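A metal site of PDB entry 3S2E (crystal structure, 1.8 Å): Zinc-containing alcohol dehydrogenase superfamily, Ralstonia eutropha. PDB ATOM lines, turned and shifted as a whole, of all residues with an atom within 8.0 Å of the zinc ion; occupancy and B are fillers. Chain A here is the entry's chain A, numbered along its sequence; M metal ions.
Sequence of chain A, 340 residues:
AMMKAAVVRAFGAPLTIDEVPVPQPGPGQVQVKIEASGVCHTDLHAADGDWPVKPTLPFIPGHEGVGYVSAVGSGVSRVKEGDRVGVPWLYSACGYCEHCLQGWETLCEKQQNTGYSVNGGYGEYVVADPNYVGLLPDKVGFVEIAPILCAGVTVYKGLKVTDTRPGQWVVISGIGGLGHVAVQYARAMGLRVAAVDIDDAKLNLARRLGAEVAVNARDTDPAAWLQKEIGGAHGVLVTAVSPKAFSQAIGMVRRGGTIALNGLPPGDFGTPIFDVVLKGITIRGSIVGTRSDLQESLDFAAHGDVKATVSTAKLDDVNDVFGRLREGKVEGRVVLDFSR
The zinc ion is bound by a ring nitrogen (NE2) of His 63 (2.0 Å), the side-chain carboxylate (OE2) of Glu 64 (2.1 Å), the side-chain sulfur (SG) of Cys 40 (2.3 Å) and the side-chain sulfur (SG) of Cys 150 (2.3 Å).
Four residues have an atom within 4 Å of the zinc ion: Cys 40, His 63, Glu 64 and Cys 150.
ND1 of His 63 lies close to OD1 of Asp 43.
The guanidinium group of Arg 333 lies within salt-bridge range of the side-chain carboxylate of Glu 64 (3.3 Å).
O of Glu 64 lies within hydrogen-bond range of N of Gly 38 (3.0 Å).
The side-chain sulfur of Cys 40 sits close to the backbone NH of Thr 42 (3.4 Å).
The side-chain carboxylate (OD2) of Asp 43 is in hydrogen-bond range of the backbone NH (N) of Cys 40 (3.0 Å).
The side-chain sulfur (SG) of Cys 150 sits close to the guanidinium group (NH1) of Arg 333 (3.6 Å).
OG1 of Thr 154 sits at hydrogen-bond distance from O of Cys 150.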
ATOM      1  N   GLY A  38       0.024   2.175  -2.402  1.00  0.00           N
ATOM      2  CA  GLY A  38       0.717   2.719  -1.237  1.00  0.00           C
ATOM      3  C   GLY A  38      -0.142   3.676  -0.418  1.00  0.00           C
ATOM      4  O   GLY A  38      -1.049   4.318  -0.962  1.00  0.00           O
ATOM      5  N   VAL A  39       0.153   3.768   0.874  1.00  0.00           N
ATOM      6  CA  VAL A  39      -0.560   4.695   1.744  1.00  0.00           C
ATOM      7  C   VAL A  39       0.423   5.710   2.284  1.00  0.00           C
ATOM      8  O   VAL A  39       1.546   5.350   2.578  1.00  0.00           O
ATOM      9  CB  VAL A  39      -1.170   3.937   2.915  1.00  0.00           C
ATOM     10  CG1 VAL A  39      -1.987   4.889   3.790  1.00  0.00           C
ATOM     11  CG2 VAL A  39      -2.074   2.829   2.385  1.00  0.00           C
ATOM     12  N   CYS A  40       0.009   6.971   2.421  1.00  0.00           N
ATOM     13  CA  CYS A  40       0.876   7.938   3.112  1.00  0.00           C
ATOM     14  C   CYS A  40       0.078   9.052   3.762  1.00  0.00           C
ATOM     15  O   CYS A  40      -1.137   9.099   3.678  1.00  0.00           O
ATOM     16  CB  CYS A  40       1.915   8.518   2.161  1.00  0.00           C
ATOM     17  SG  CYS A  40       1.236   9.796   1.086  1.00  0.00           S
ATOM     18  N   HIS A  41       0.780   9.962   4.426  1.00  0.00           N
ATOM     19  CA  HIS A  41       0.075  11.032   5.120  1.00  0.00           C
ATOM     20  C   HIS A  41      -0.801  11.911   4.236  1.00  0.00           C
ATOM     21  O   HIS A  41      -1.763  12.486   4.707  1.00  0.00           O
ATOM     22  CB  HIS A  41       1.068  11.893   5.900  1.00  0.00           C
ATOM     23  CG  HIS A  41       1.403  11.344   7.251  1.00  0.00           C
ATOM     24  ND1 HIS A  41       2.330  10.332   7.440  1.00  0.00           N
ATOM     25  CD2 HIS A  41       0.923  11.652   8.483  1.00  0.00           C
ATOM     26  CE1 HIS A  41       2.414  10.062   8.730  1.00  0.00           C
ATOM     27  NE2 HIS A  41       1.572  10.838   9.386  1.00  0.00           N
ATOM     28  N   THR A  42      -0.442  12.035   2.960  1.00  0.00           N
ATOM     29  CA  THR A  42      -1.268  12.814   2.044  1.00  0.00           C
ATOM     30  C   THR A  42      -2.688  12.256   2.009  1.00  0.00           C
ATOM     31  O   THR A  42      -3.654  13.014   1.900  1.00  0.00           O
ATOM     32  CB  THR A  42      -0.613  12.899   0.642  1.00  0.00           C
ATOM     33  OG1 THR A  42       0.559  13.719   0.752  1.00  0.00           O
ATOM     34  CG2 THR A  42      -1.589  13.484  -0.387  1.00  0.00           C
ATOM     35  N   ASP A  43      -2.823  10.925   2.134  1.00  0.00           N
ATOM     36  CA  ASP A  43      -4.140  10.292   2.116  1.00  0.00           C
ATOM     37  C   ASP A  43      -4.975  10.712   3.329  1.00  0.00           C
ATOM     38  O   ASP A  43      -6.187  10.828   3.207  1.00  0.00           O
ATOM     39  CB  ASP A  43      -4.047   8.758   2.052  1.00  0.00           C
ATOM     40  CG  ASP A  43      -3.299   8.278   0.805  1.00  0.00           C
ATOM     41  OD1 ASP A  43      -3.449   8.931  -0.252  1.00  0.00           O
ATOM     42  OD2 ASP A  43      -2.579   7.263   0.887  1.00  0.00           O
ATOM     43  N   GLY A  62      -5.866   7.569  -2.922  1.00  0.00           N
ATOM     44  CA  GLY A  62      -4.760   6.711  -3.340  1.00  0.00           C
ATOM     45  C   GLY A  62      -4.028   7.226  -4.573  1.00  0.00           C
ATOM     46  O   GLY A  62      -4.536   7.111  -5.674  1.00  0.00           O
ATOM     47  N   HIS A  63      -2.833   7.773  -4.376  1.00  0.00           N
ATOM     48  CA  HIS A  63      -2.021   8.259  -5.494  1.00  0.00           C
ATOM     49  C   HIS A  63      -0.768   7.399  -5.635  1.00  0.00           C
ATOM     50  O   HIS A  63       0.254   7.845  -6.164  1.00  0.00           O
ATOM     51  CB  HIS A  63      -1.578   9.710  -5.233  1.00  0.00           C
ATOM     52  CG  HIS A  63      -0.944   9.875  -3.899  1.00  0.00           C
ATOM     53  ND1 HIS A  63      -1.677  10.065  -2.755  1.00  0.00           N
ATOM     54  CD2 HIS A  63       0.355   9.785  -3.509  1.00  0.00           C
ATOM     55  CE1 HIS A  63      -0.868  10.133  -1.714  1.00  0.00           C
ATOM     56  NE2 HIS A  63       0.382   9.961  -2.142  1.00  0.00           N
ATOM     57  N   GLU A  64      -0.820   6.170  -5.131  1.00  0.00           N
ATOM     58  CA  GLU A  64       0.343   5.284  -5.243  1.00  0.00           C
ATOM     59  C   GLU A  64      -0.068   3.892  -5.726  1.00  0.00           C
ATOM     60  O   GLU A  64       0.484   2.874  -5.284  1.00  0.00           O
ATOM     61  CB  GLU A  64       1.032   5.148  -3.899  1.00  0.00           C
ATOM     62  CG  GLU A  64       1.559   6.466  -3.314  1.00  0.00           C
ATOM     63  CD  GLU A  64       2.271   6.284  -1.996  1.00  0.00           C
ATOM     64  OE1 GLU A  64       2.816   5.211  -1.722  1.00  0.00           O
ATOM     65  OE2 GLU A  64       2.283   7.232  -1.188  1.00  0.00           O
ATOM     66  N   TRP A  89       0.435  10.905  -8.119  1.00  0.00           N
ATOM     67  CA  TRP A  89      -0.248  12.143  -7.763  1.00  0.00           C
ATOM     68  C   TRP A  89      -0.620  13.027  -8.943  1.00  0.00           C
ATOM     69  O   TRP A  89      -1.752  13.537  -9.043  1.00  0.00           O
ATOM     70  CB  TRP A  89       0.646  12.924  -6.797  1.00  0.00           C
ATOM     71  CG  TRP A  89       0.139  14.299  -6.389  1.00  0.00           C
ATOM     72  CD1 TRP A  89       0.653  15.513  -6.784  1.00  0.00           C
ATOM     73  CD2 TRP A  89      -0.918  14.601  -5.462  1.00  0.00           C
ATOM     74  NE1 TRP A  89      -0.035  16.548  -6.166  1.00  0.00           N
ATOM     75  CE2 TRP A  89      -0.995  16.013  -5.344  1.00  0.00           C
ATOM     76  CE3 TRP A  89      -1.800  13.818  -4.716  1.00  0.00           C
ATOM     77  CZ2 TRP A  89      -1.929  16.657  -4.514  1.00  0.00           C
ATOM     78  CZ3 TRP A  89      -2.741  14.463  -3.894  1.00  0.00           C
ATOM     79  CH2 TRP A  89      -2.790  15.860  -3.803  1.00  0.00           C
ATOM     80  N   TYR A 122      -7.288   3.272  -4.267  1.00  0.00           N
ATOM     81  CA  TYR A 122      -7.772   2.444  -3.142  1.00  0.00           C
ATOM     82  C   TYR A 122      -8.958   1.603  -3.619  1.00  0.00           C
ATOM     83  O   TYR A 122     -10.005   1.529  -2.969  1.00  0.00           O
ATOM     84  CB  TYR A 122      -8.242   3.295  -1.943  1.00  0.00           C
ATOM     85  CG  TYR A 122      -7.179   3.866  -1.026  1.00  0.00           C
ATOM     86  CD1 TYR A 122      -7.512   4.346   0.251  1.00  0.00           C
ATOM     87  CD2 TYR A 122      -5.839   3.956  -1.413  1.00  0.00           C
ATOM     88  CE1 TYR A 122      -6.552   4.890   1.112  1.00  0.00           C
ATOM     89  CE2 TYR A 122      -4.864   4.509  -0.537  1.00  0.00           C
ATOM     90  CZ  TYR A 122      -5.242   4.974   0.711  1.00  0.00           C
ATOM     91  OH  TYR A 122      -4.303   5.522   1.579  1.00  0.00           O
ATOM     92  N   ALA A 146       5.634   0.641  -5.191  1.00  0.00           N
ATOM     93  CA  ALA A 146       4.562   1.616  -5.032  1.00  0.00           C
ATOM     94  C   ALA A 146       5.033   2.944  -4.391  1.00  0.00           C
ATOM     95  O   ALA A 146       4.705   4.017  -4.905  1.00  0.00           O
ATOM     96  CB  ALA A 146       3.366   1.024  -4.223  1.00  0.00           C
ATOM     97  N   PRO A 147       5.784   2.871  -3.282  1.00  0.00           N
ATOM     98  CA  PRO A 147       6.121   4.158  -2.655  1.00  0.00           C
ATOM     99  C   PRO A 147       7.072   5.019  -3.474  1.00  0.00           C
ATOM    100  O   PRO A 147       7.197   6.214  -3.198  1.00  0.00           O
ATOM    101  CB  PRO A 147       6.787   3.771  -1.343  1.00  0.00           C
ATOM    102  CG  PRO A 147       6.406   2.329  -1.102  1.00  0.00           C
ATOM    103  CD  PRO A 147       6.140   1.714  -2.439  1.00  0.00           C
ATOM    104  N   LEU A 149       6.552   5.956  -6.354  1.00  0.00           N
ATOM    105  CA  LEU A 149       5.656   6.905  -7.043  1.00  0.00           C
ATOM    106  C   LEU A 149       5.410   8.184  -6.241  1.00  0.00           C
ATOM    107  O   LEU A 149       4.915   9.190  -6.781  1.00  0.00           O
ATOM    108  CB  LEU A 149       4.266   6.295  -7.295  1.00  0.00           C
ATOM    109  CG  LEU A 149       4.176   5.063  -8.185  1.00  0.00           C
ATOM    110  CD1 LEU A 149       2.714   4.597  -8.365  1.00  0.00           C
ATOM    111  CD2 LEU A 149       4.814   5.375  -9.531  1.00  0.00           C
ATOM    112  N   CYS A 150       5.742   8.140  -4.957  1.00  0.00           N
ATOM    113  CA  CYS A 150       5.434   9.250  -4.043  1.00  0.00           C
ATOM    114  C   CYS A 150       6.683   9.708  -3.276  1.00  0.00           C
ATOM    115  O   CYS A 150       7.280  10.770  -3.602  1.00  0.00           O
ATOM    116  CB  CYS A 150       4.268   8.871  -3.100  1.00  0.00           C
ATOM    117  SG  CYS A 150       3.999  10.120  -1.816  1.00  0.00           S
ATOM    118  N   ALA A 151       7.098   8.912  -2.284  1.00  0.00           N
ATOM    119  CA  ALA A 151       8.287   9.217  -1.505  1.00  0.00           C
ATOM    120  C   ALA A 151       9.503   9.306  -2.430  1.00  0.00           C
ATOM    121  O   ALA A 151      10.350  10.195  -2.303  1.00  0.00           O
ATOM    122  CB  ALA A 151       8.524   8.136  -0.453  1.00  0.00           C
ATOM    123  N   THR A 154       9.468  12.318  -4.951  1.00  0.00           N
ATOM    124  CA  THR A 154       9.550  13.538  -4.153  1.00  0.00           C
ATOM    125  C   THR A 154      10.966  13.860  -3.635  1.00  0.00           C
ATOM    126  O   THR A 154      11.450  14.986  -3.801  1.00  0.00           O
ATOM    127  CB  THR A 154       8.542  13.517  -2.974  1.00  0.00           C
ATOM    128  OG1 THR A 154       7.214  13.688  -3.495  1.00  0.00           O
ATOM    129  CG2 THR A 154       8.834  14.671  -2.010  1.00  0.00           C
ATOM    130  N   LEU A 178       9.786   9.598   4.169  1.00  0.00           N
ATOM    131  CA  LEU A 178      10.556  10.182   3.061  1.00  0.00           C
ATOM    132  C   LEU A 178      12.076  10.084   3.290  1.00  0.00           C
ATOM    133  O   LEU A 178      12.846   9.725   2.386  1.00  0.00           O
ATOM    134  CB  LEU A 178      10.201  11.675   2.872  1.00  0.00           C
ATOM    135  CG  LEU A 178       8.831  12.094   2.335  1.00  0.00           C
ATOM    136  CD1 LEU A 178       8.961  13.446   1.629  1.00  0.00           C
ATOM    137  CD2 LEU A 178       8.322  11.064   1.401  1.00  0.00           C
ATOM    138  N   VAL A 288       6.719  16.022  -5.095  1.00  0.00           N
ATOM    139  CA  VAL A 288       6.619  15.136  -6.259  1.00  0.00           C
ATOM    140  C   VAL A 288       7.585  15.508  -7.373  1.00  0.00           C
ATOM    141  O   VAL A 288       8.719  15.935  -7.101  1.00  0.00           O
ATOM    142  CB  VAL A 288       5.147  14.923  -6.767  1.00  0.00           C
ATOM    143  CG1 VAL A 288       4.247  14.471  -5.615  1.00  0.00           C
ATOM    144  CG2 VAL A 288       4.607  16.194  -7.430  1.00  0.00           C
ATOM    145  N   ARG A 333       6.895   2.635   5.045  1.00  0.00           N
ATOM    146  CA  ARG A 333       5.656   2.865   4.331  1.00  0.00           C
ATOM    147  C   ARG A 333       4.775   1.613   4.394  1.00  0.00           C
ATOM    148  O   ARG A 333       5.303   0.501   4.358  1.00  0.00           O
ATOM    149  CB  ARG A 333       5.952   3.225   2.876  1.00  0.00           C
ATOM    150  CG  ARG A 333       6.412   4.667   2.670  1.00  0.00           C
ATOM    151  CD  ARG A 333       5.256   5.610   3.007  1.00  0.00           C
ATOM    152  NE  ARG A 333       5.482   7.009   2.618  1.00  0.00           N
ATOM    153  CZ  ARG A 333       5.211   7.514   1.424  1.00  0.00           C
ATOM    154  NH1 ARG A 333       5.421   8.810   1.195  1.00  0.00           N
ATOM    155  NH2 ARG A 333       4.733   6.741   0.445  1.00  0.00           N
HETATM  156 ZN    ZN M   1       1.959   9.288  -1.051  1.00  0.00          ZN
